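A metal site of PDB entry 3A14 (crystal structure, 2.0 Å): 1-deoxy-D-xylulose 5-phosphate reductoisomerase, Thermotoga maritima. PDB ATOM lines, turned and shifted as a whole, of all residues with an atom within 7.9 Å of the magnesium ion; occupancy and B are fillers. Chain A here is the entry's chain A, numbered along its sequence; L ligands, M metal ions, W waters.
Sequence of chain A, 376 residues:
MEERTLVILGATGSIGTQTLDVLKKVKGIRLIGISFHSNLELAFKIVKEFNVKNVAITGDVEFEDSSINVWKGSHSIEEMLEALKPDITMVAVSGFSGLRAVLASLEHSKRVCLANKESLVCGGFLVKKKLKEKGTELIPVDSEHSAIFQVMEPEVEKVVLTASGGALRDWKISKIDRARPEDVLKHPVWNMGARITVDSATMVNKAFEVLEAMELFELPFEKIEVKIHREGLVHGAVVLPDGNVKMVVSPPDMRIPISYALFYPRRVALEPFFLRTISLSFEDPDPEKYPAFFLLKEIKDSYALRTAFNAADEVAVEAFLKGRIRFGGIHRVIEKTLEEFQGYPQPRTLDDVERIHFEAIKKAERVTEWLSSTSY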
ATOM      1  N   LYS A 117     -12.739  -8.021  -6.006  1.00  0.00           N
ATOM      2  CA  LYS A 117     -13.311  -8.933  -5.011  1.00  0.00           C
ATOM      3  C   LYS A 117     -14.680  -8.492  -4.476  1.00  0.00           C
ATOM      4  O   LYS A 117     -15.532  -9.343  -4.168  1.00  0.00           O
ATOM      5  CB  LYS A 117     -12.351  -9.080  -3.827  1.00  0.00           C
ATOM      6  CG  LYS A 117     -10.959  -9.572  -4.220  1.00  0.00           C
ATOM      7  CD  LYS A 117     -10.273 -10.259  -3.023  1.00  0.00           C
ATOM      8  CE  LYS A 117      -8.895 -10.732  -3.383  1.00  0.00           C
ATOM      9  NZ  LYS A 117      -8.958 -11.798  -4.411  1.00  0.00           N
ATOM     10  N   VAL A 141      -8.967 -13.686 -11.933  1.00  0.00           N
ATOM     11  CA  VAL A 141      -7.560 -13.290 -12.086  1.00  0.00           C
ATOM     12  C   VAL A 141      -6.786 -13.558 -10.772  1.00  0.00           C
ATOM     13  O   VAL A 141      -5.576 -13.772 -10.785  1.00  0.00           O
ATOM     14  CB  VAL A 141      -7.438 -11.809 -12.577  1.00  0.00           C
ATOM     15  CG1 VAL A 141      -6.006 -11.328 -12.561  1.00  0.00           C
ATOM     16  CG2 VAL A 141      -8.012 -11.677 -13.984  1.00  0.00           C
ATOM     17  N   ASP A 142      -7.471 -13.542  -9.641  1.00  0.00           N
ATOM     18  CA  ASP A 142      -6.831 -13.815  -8.333  1.00  0.00           C
ATOM     19  C   ASP A 142      -6.016 -15.091  -8.424  1.00  0.00           C
ATOM     20  O   ASP A 142      -6.508 -16.055  -8.971  1.00  0.00           O
ATOM     21  CB  ASP A 142      -7.943 -13.979  -7.294  1.00  0.00           C
ATOM     22  CG  ASP A 142      -7.409 -14.337  -5.932  1.00  0.00           C
ATOM     23  OD1 ASP A 142      -7.034 -13.416  -5.176  1.00  0.00           O
ATOM     24  OD2 ASP A 142      -7.404 -15.546  -5.617  1.00  0.00           O
ATOM     25  N   SER A 143      -4.792 -15.120  -7.889  1.00  0.00           N
ATOM     26  CA  SER A 143      -3.898 -16.237  -8.108  1.00  0.00           C
ATOM     27  C   SER A 143      -4.447 -17.524  -7.518  1.00  0.00           C
ATOM     28  O   SER A 143      -4.286 -18.586  -8.110  1.00  0.00           O
ATOM     29  CB  SER A 143      -2.496 -15.932  -7.544  1.00  0.00           C
ATOM     30  OG  SER A 143      -2.552 -15.953  -6.124  1.00  0.00           O
ATOM     31  N   GLU A 144      -5.097 -17.437  -6.361  1.00  0.00           N
ATOM     32  CA  GLU A 144      -5.666 -18.623  -5.709  1.00  0.00           C
ATOM     33  C   GLU A 144      -6.885 -19.151  -6.513  1.00  0.00           C
ATOM     34  O   GLU A 144      -7.020 -20.361  -6.727  1.00  0.00           O
ATOM     35  CB  GLU A 144      -6.068 -18.328  -4.248  1.00  0.00           C
ATOM     36  CG  GLU A 144      -4.881 -18.093  -3.290  1.00  0.00           C
ATOM     37  CD  GLU A 144      -4.370 -16.657  -3.293  1.00  0.00           C
ATOM     38  OE1 GLU A 144      -4.930 -15.791  -4.019  1.00  0.00           O
ATOM     39  OE2 GLU A 144      -3.399 -16.361  -2.557  1.00  0.00           O
ATOM     40  N   HIS A 145      -7.754 -18.266  -6.969  1.00  0.00           N
ATOM     41  CA  HIS A 145      -8.933 -18.758  -7.748  1.00  0.00           C
ATOM     42  C   HIS A 145      -8.526 -19.242  -9.152  1.00  0.00           C
ATOM     43  O   HIS A 145      -9.115 -20.156  -9.712  1.00  0.00           O
ATOM     44  CB  HIS A 145     -10.017 -17.712  -7.848  1.00  0.00           C
ATOM     45  CG  HIS A 145     -10.444 -17.149  -6.529  1.00  0.00           C
ATOM     46  ND1 HIS A 145     -10.524 -15.787  -6.289  1.00  0.00           N
ATOM     47  CD2 HIS A 145     -10.795 -17.757  -5.375  1.00  0.00           C
ATOM     48  CE1 HIS A 145     -10.907 -15.594  -5.037  1.00  0.00           C
ATOM     49  NE2 HIS A 145     -11.080 -16.762  -4.460  1.00  0.00           N
ATOM     50  N   THR A 162      -4.452 -21.098   0.034  1.00  0.00           N
ATOM     51  CA  THR A 162      -3.261 -20.876   0.872  1.00  0.00           C
ATOM     52  C   THR A 162      -3.138 -19.396   1.175  1.00  0.00           C
ATOM     53  O   THR A 162      -3.700 -18.570   0.458  1.00  0.00           O
ATOM     54  CB  THR A 162      -1.984 -21.352   0.165  1.00  0.00           C
ATOM     55  OG1 THR A 162      -1.960 -20.809  -1.146  1.00  0.00           O
ATOM     56  CG2 THR A 162      -1.950 -22.895   0.096  1.00  0.00           C
ATOM     57  N   ILE A 196      -4.425  -3.882   0.285  1.00  0.00           N
ATOM     58  CA  ILE A 196      -4.226  -5.305   0.097  1.00  0.00           C
ATOM     59  C   ILE A 196      -3.237  -5.830   1.118  1.00  0.00           C
ATOM     60  O   ILE A 196      -3.450  -6.882   1.730  1.00  0.00           O
ATOM     61  CB  ILE A 196      -3.778  -5.650  -1.350  1.00  0.00           C
ATOM     62  CG1 ILE A 196      -5.001  -5.642  -2.266  1.00  0.00           C
ATOM     63  CG2 ILE A 196      -3.079  -7.008  -1.410  1.00  0.00           C
ATOM     64  CD1 ILE A 196      -4.683  -5.263  -3.705  1.00  0.00           C
ATOM     65  N   SER A 200      -4.053  -8.556   4.046  1.00  0.00           N
ATOM     66  CA  SER A 200      -3.285  -9.806   4.178  1.00  0.00           C
ATOM     67  C   SER A 200      -2.807 -10.028   5.608  1.00  0.00           C
ATOM     68  O   SER A 200      -2.657 -11.169   6.071  1.00  0.00           O
ATOM     69  CB  SER A 200      -2.080  -9.806   3.224  1.00  0.00           C
ATOM     70  OG  SER A 200      -2.499  -9.317   1.957  1.00  0.00           O
ATOM     71  N   ASN A 205      -8.365 -10.274   3.595  1.00  0.00           N
ATOM     72  CA  ASN A 205      -8.276 -10.620   2.155  1.00  0.00           C
ATOM     73  C   ASN A 205      -8.592 -12.096   1.907  1.00  0.00           C
ATOM     74  O   ASN A 205      -9.260 -12.441   0.931  1.00  0.00           O
ATOM     75  CB  ASN A 205      -6.901 -10.289   1.607  1.00  0.00           C
ATOM     76  CG  ASN A 205      -6.854 -10.395   0.103  1.00  0.00           C
ATOM     77  OD1 ASN A 205      -7.457  -9.581  -0.610  1.00  0.00           O
ATOM     78  ND2 ASN A 205      -6.156 -11.414  -0.390  1.00  0.00           N
ATOM     79  N   LYS A 206      -8.107 -12.947   2.796  1.00  0.00           N
ATOM     80  CA  LYS A 206      -8.392 -14.361   2.696  1.00  0.00           C
ATOM     81  C   LYS A 206      -9.861 -14.683   2.952  1.00  0.00           C
ATOM     82  O   LYS A 206     -10.402 -15.596   2.345  1.00  0.00           O
ATOM     83  CB  LYS A 206      -7.453 -15.186   3.581  1.00  0.00           C
ATOM     84  CG  LYS A 206      -7.209 -16.602   3.119  1.00  0.00           C
ATOM     85  CD  LYS A 206      -6.710 -16.723   1.668  1.00  0.00           C
ATOM     86  CE  LYS A 206      -5.585 -15.785   1.370  1.00  0.00           C
ATOM     87  NZ  LYS A 206      -4.867 -16.063   0.105  1.00  0.00           N
ATOM     88  N   GLU A 209     -11.577 -14.027  -0.205  1.00  0.00           N
ATOM     89  CA  GLU A 209     -11.292 -15.093  -1.175  1.00  0.00           C
ATOM     90  C   GLU A 209     -12.117 -16.352  -0.954  1.00  0.00           C
ATOM     91  O   GLU A 209     -12.517 -17.014  -1.918  1.00  0.00           O
ATOM     92  CB  GLU A 209      -9.796 -15.407  -1.234  1.00  0.00           C
ATOM     93  CG  GLU A 209      -8.978 -14.267  -1.808  1.00  0.00           C
ATOM     94  CD  GLU A 209      -7.491 -14.610  -1.884  1.00  0.00           C
ATOM     95  OE1 GLU A 209      -7.102 -15.683  -1.397  1.00  0.00           O
ATOM     96  OE2 GLU A 209      -6.697 -13.813  -2.455  1.00  0.00           O
ATOM     97  N   GLU A 212     -15.505 -15.399  -2.325  1.00  0.00           N
ATOM     98  CA  GLU A 212     -15.353 -15.475  -3.806  1.00  0.00           C
ATOM     99  C   GLU A 212     -15.315 -16.897  -4.363  1.00  0.00           C
ATOM    100  O   GLU A 212     -15.966 -17.202  -5.367  1.00  0.00           O
ATOM    101  CB  GLU A 212     -14.126 -14.731  -4.225  1.00  0.00           C
ATOM    102  CG  GLU A 212     -14.232 -13.251  -4.086  1.00  0.00           C
ATOM    103  CD  GLU A 212     -13.005 -12.593  -4.640  1.00  0.00           C
ATOM    104  OE1 GLU A 212     -13.009 -12.288  -5.845  1.00  0.00           O
ATOM    105  OE2 GLU A 212     -12.017 -12.456  -3.871  1.00  0.00           O
ATOM    106  N   HIS A 235      -0.611 -22.386  -4.813  1.00  0.00           N
ATOM    107  CA  HIS A 235      -1.652 -21.342  -4.919  1.00  0.00           C
ATOM    108  C   HIS A 235      -3.058 -21.900  -4.774  1.00  0.00           C
ATOM    109  O   HIS A 235      -4.003 -21.155  -4.628  1.00  0.00           O
ATOM    110  CB  HIS A 235      -1.490 -20.505  -6.209  1.00  0.00           C
ATOM    111  CG  HIS A 235      -0.166 -19.804  -6.284  1.00  0.00           C
ATOM    112  ND1 HIS A 235       0.196 -18.825  -5.386  1.00  0.00           N
ATOM    113  CD2 HIS A 235       0.902 -19.999  -7.075  1.00  0.00           C
ATOM    114  CE1 HIS A 235       1.418 -18.410  -5.664  1.00  0.00           C
ATOM    115  NE2 HIS A 235       1.877 -19.115  -6.671  1.00  0.00           N
ATOM    116  N   MET A 254       1.735 -12.072 -10.443  1.00  0.00           N
ATOM    117  CA  MET A 254       0.329 -11.943 -10.904  1.00  0.00           C
ATOM    118  C   MET A 254       0.215 -11.935 -12.414  1.00  0.00           C
ATOM    119  O   MET A 254      -0.888 -12.113 -12.944  1.00  0.00           O
ATOM    120  CB  MET A 254      -0.322 -10.686 -10.311  1.00  0.00           C
ATOM    121  CG  MET A 254      -0.774 -10.802  -8.837  1.00  0.00           C
ATOM    122  SD  MET A 254      -1.830 -12.229  -8.536  1.00  0.00           S
ATOM    123  CE  MET A 254      -3.299 -11.865  -9.515  1.00  0.00           C
HETATM  124  P1  LIG L   1      -5.228  -0.492  -7.105  1.00  0.00           P
HETATM  125  O1  LIG L   1      -5.628   0.478  -6.035  1.00  0.00           O
HETATM  126  O2  LIG L   1      -3.626  -0.750  -7.229  1.00  0.00           O
HETATM  127  O3  LIG L   1      -5.840  -0.028  -8.546  1.00  0.00           O
HETATM  128  C1  LIG L   1      -7.234  -0.219  -8.841  1.00  0.00           C
HETATM  129  C2  LIG L   1      -7.758   0.679  -9.985  1.00  0.00           C
HETATM  130  O4  LIG L   1      -9.141   1.083  -9.657  1.00  0.00           O
HETATM  131  C3  LIG L   1      -6.981   1.989 -10.266  1.00  0.00           C
HETATM  132  O5  LIG L   1      -6.998   2.261 -11.696  1.00  0.00           O
HETATM  133  C4  LIG L   1      -7.820   3.046  -9.595  1.00  0.00           C
HETATM  134  O6  LIG L   1      -7.686   4.292 -10.315  1.00  0.00           O
HETATM  135  C5  LIG L   1      -9.219   2.500  -9.877  1.00  0.00           C
HETATM  136  N1  LIG L   1     -10.236   3.046  -8.940  1.00  0.00           N
HETATM  137  C6  LIG L   1     -10.002   3.465  -7.688  1.00  0.00           C
HETATM  138  N2  LIG L   1     -11.160   3.875  -7.159  1.00  0.00           N
HETATM  139  C7  LIG L   1     -12.107   3.735  -8.082  1.00  0.00           C
HETATM  140  C8  LIG L   1     -13.467   3.996  -8.094  1.00  0.00           C
HETATM  141  N3  LIG L   1     -14.047   4.501  -6.997  1.00  0.00           N
HETATM  142  N4  LIG L   1     -14.166   3.730  -9.208  1.00  0.00           N
HETATM  143  C9  LIG L   1     -13.588   3.215 -10.301  1.00  0.00           C
HETATM  144  N5  LIG L   1     -12.281   2.953 -10.318  1.00  0.00           N
HETATM  145  C10 LIG L   1     -11.531   3.199  -9.221  1.00  0.00           C
HETATM  146  O7  LIG L   1      -5.920  -1.949  -6.829  1.00  0.00           O
HETATM  147  P2  LIG L   1      -5.335  -3.380  -7.391  1.00  0.00           P
HETATM  148  O8  LIG L   1      -4.197  -3.882  -6.584  1.00  0.00           O
HETATM  149  O9  LIG L   1      -5.020  -3.363  -9.002  1.00  0.00           O
HETATM  150  O10 LIG L   1      -6.638  -4.346  -7.268  1.00  0.00           O
HETATM  151  C11 LIG L   1      -7.961  -3.990  -7.709  1.00  0.00           C
HETATM  152  C12 LIG L   1      -8.905  -5.141  -7.365  1.00  0.00           C
HETATM  153  O11 LIG L   1      -8.149  -6.347  -7.772  1.00  0.00           O
HETATM  154  C13 LIG L   1      -9.164  -5.259  -5.846  1.00  0.00           C
HETATM  155  O12 LIG L   1     -10.542  -5.623  -5.586  1.00  0.00           O
HETATM  156  C14 LIG L   1      -8.192  -6.383  -5.437  1.00  0.00           C
HETATM  157  O13 LIG L   1      -8.632  -7.104  -4.282  1.00  0.00           O
HETATM  158  C15 LIG L   1      -8.203  -7.288  -6.674  1.00  0.00           C
HETATM  159  N6  LIG L   1      -7.010  -8.161  -6.629  1.00  0.00           N
HETATM  160  C16 LIG L   1      -5.732  -7.587  -6.541  1.00  0.00           C
HETATM  161  C17 LIG L   1      -4.602  -8.399  -6.471  1.00  0.00           C
HETATM  162  C18 LIG L   1      -3.217  -7.754  -6.369  1.00  0.00           C
HETATM  163  O14 LIG L   1      -2.205  -8.453  -6.313  1.00  0.00           O
HETATM  164  N7  LIG L   1      -3.191  -6.416  -6.347  1.00  0.00           N
HETATM  165  C19 LIG L   1      -4.728  -9.946  -6.511  1.00  0.00           C
HETATM  166  C20 LIG L   1      -6.051 -10.412  -6.607  1.00  0.00           C
HETATM  167  C21 LIG L   1      -7.170  -9.562  -6.663  1.00  0.00           C
HETATM  168  P3  LIG L   1      -6.564   5.428  -9.926  1.00  0.00           P
HETATM  169  O15 LIG L   1      -5.225   4.885  -9.611  1.00  0.00           O
HETATM  170  O16 LIG L   1      -6.575   6.435 -11.181  1.00  0.00           O
HETATM  171  O17 LIG L   1      -7.119   6.303  -8.703  1.00  0.00           O
HETATM  172 MG    MG M   1      -5.187 -13.917  -3.743  1.00  0.00          MG
HETATM  173  O   HOH W   1      -3.768 -13.688  -1.910  1.00  0.00           O
HETATM  174  O   HOH W   2      -5.576 -11.427  -3.738  1.00  0.00           O
HETATM  175  O   HOH W   3      -3.928 -12.910  -5.970  1.00  0.00           O
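The backbone NH (N) of Lys 117 lies within hydrogen-bond range of an oxygen (O12) of the ligand (3.3 Å).
The side-chain carboxylate of Glu 209 is in salt-bridge range of the side-chain amino group of Lys 206 (2.7 Å). The side-chain carboxylate of Glu 209 sits close to the side-chain amide nitrogen of Asn 205. The backbone NH of His 145 is in hydrogen-bond range of the side-chain carboxylate of Asp 142. OD1 of Asp 142 sits close to NZ of Lys 117. The side-chain carboxylate of Glu 144 lies close to the side-chain hydroxyl of Ser 143 (3.2 Å). The backbone carbonyl oxygen (O) of Glu 209 sits at hydrogen-bond distance from a ring nitrogen (NE2) of His 145. The side-chain carboxylate (OE2) of Glu 209 sits close to the side-chain amino group (NZ) of Lys 117, 3.6 Å away. The side-chain carboxylate (OE2) of Glu 144 is in salt-bridge range of the side-chain amino group (NZ) of Lys 206 (3.1 Å).
Three residues have an atom within 4 Å of the magnesium ion: Asp 142, Glu 144 and Glu 209.
The magnesium ion is bound by the side-chain carboxylate (OE1) of Glu 144 (1.9 Å), the side-chain carboxylate (OE2) of Glu 209 (2.0 Å), water W1 (2.3 Å), the side-chain carboxylate (OD1) of Asp 142 (2.4 Å) and water W2 (2.5 Å). The magnesium ion has five donor atoms within binding distance. Slightly farther from the magnesium ion lies water W3 (2.7 Å).
Water W1 lies within hydrogen-bond range of OE2 of Glu 144 and NZ of Lys 206. Water W2 lies within hydrogen-bond range of ND2 of Asn 205 and NZ of Lys 117. Water W3 bridges the backbone NH of Ser 143 and the side-chain sulfur of Met 254.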
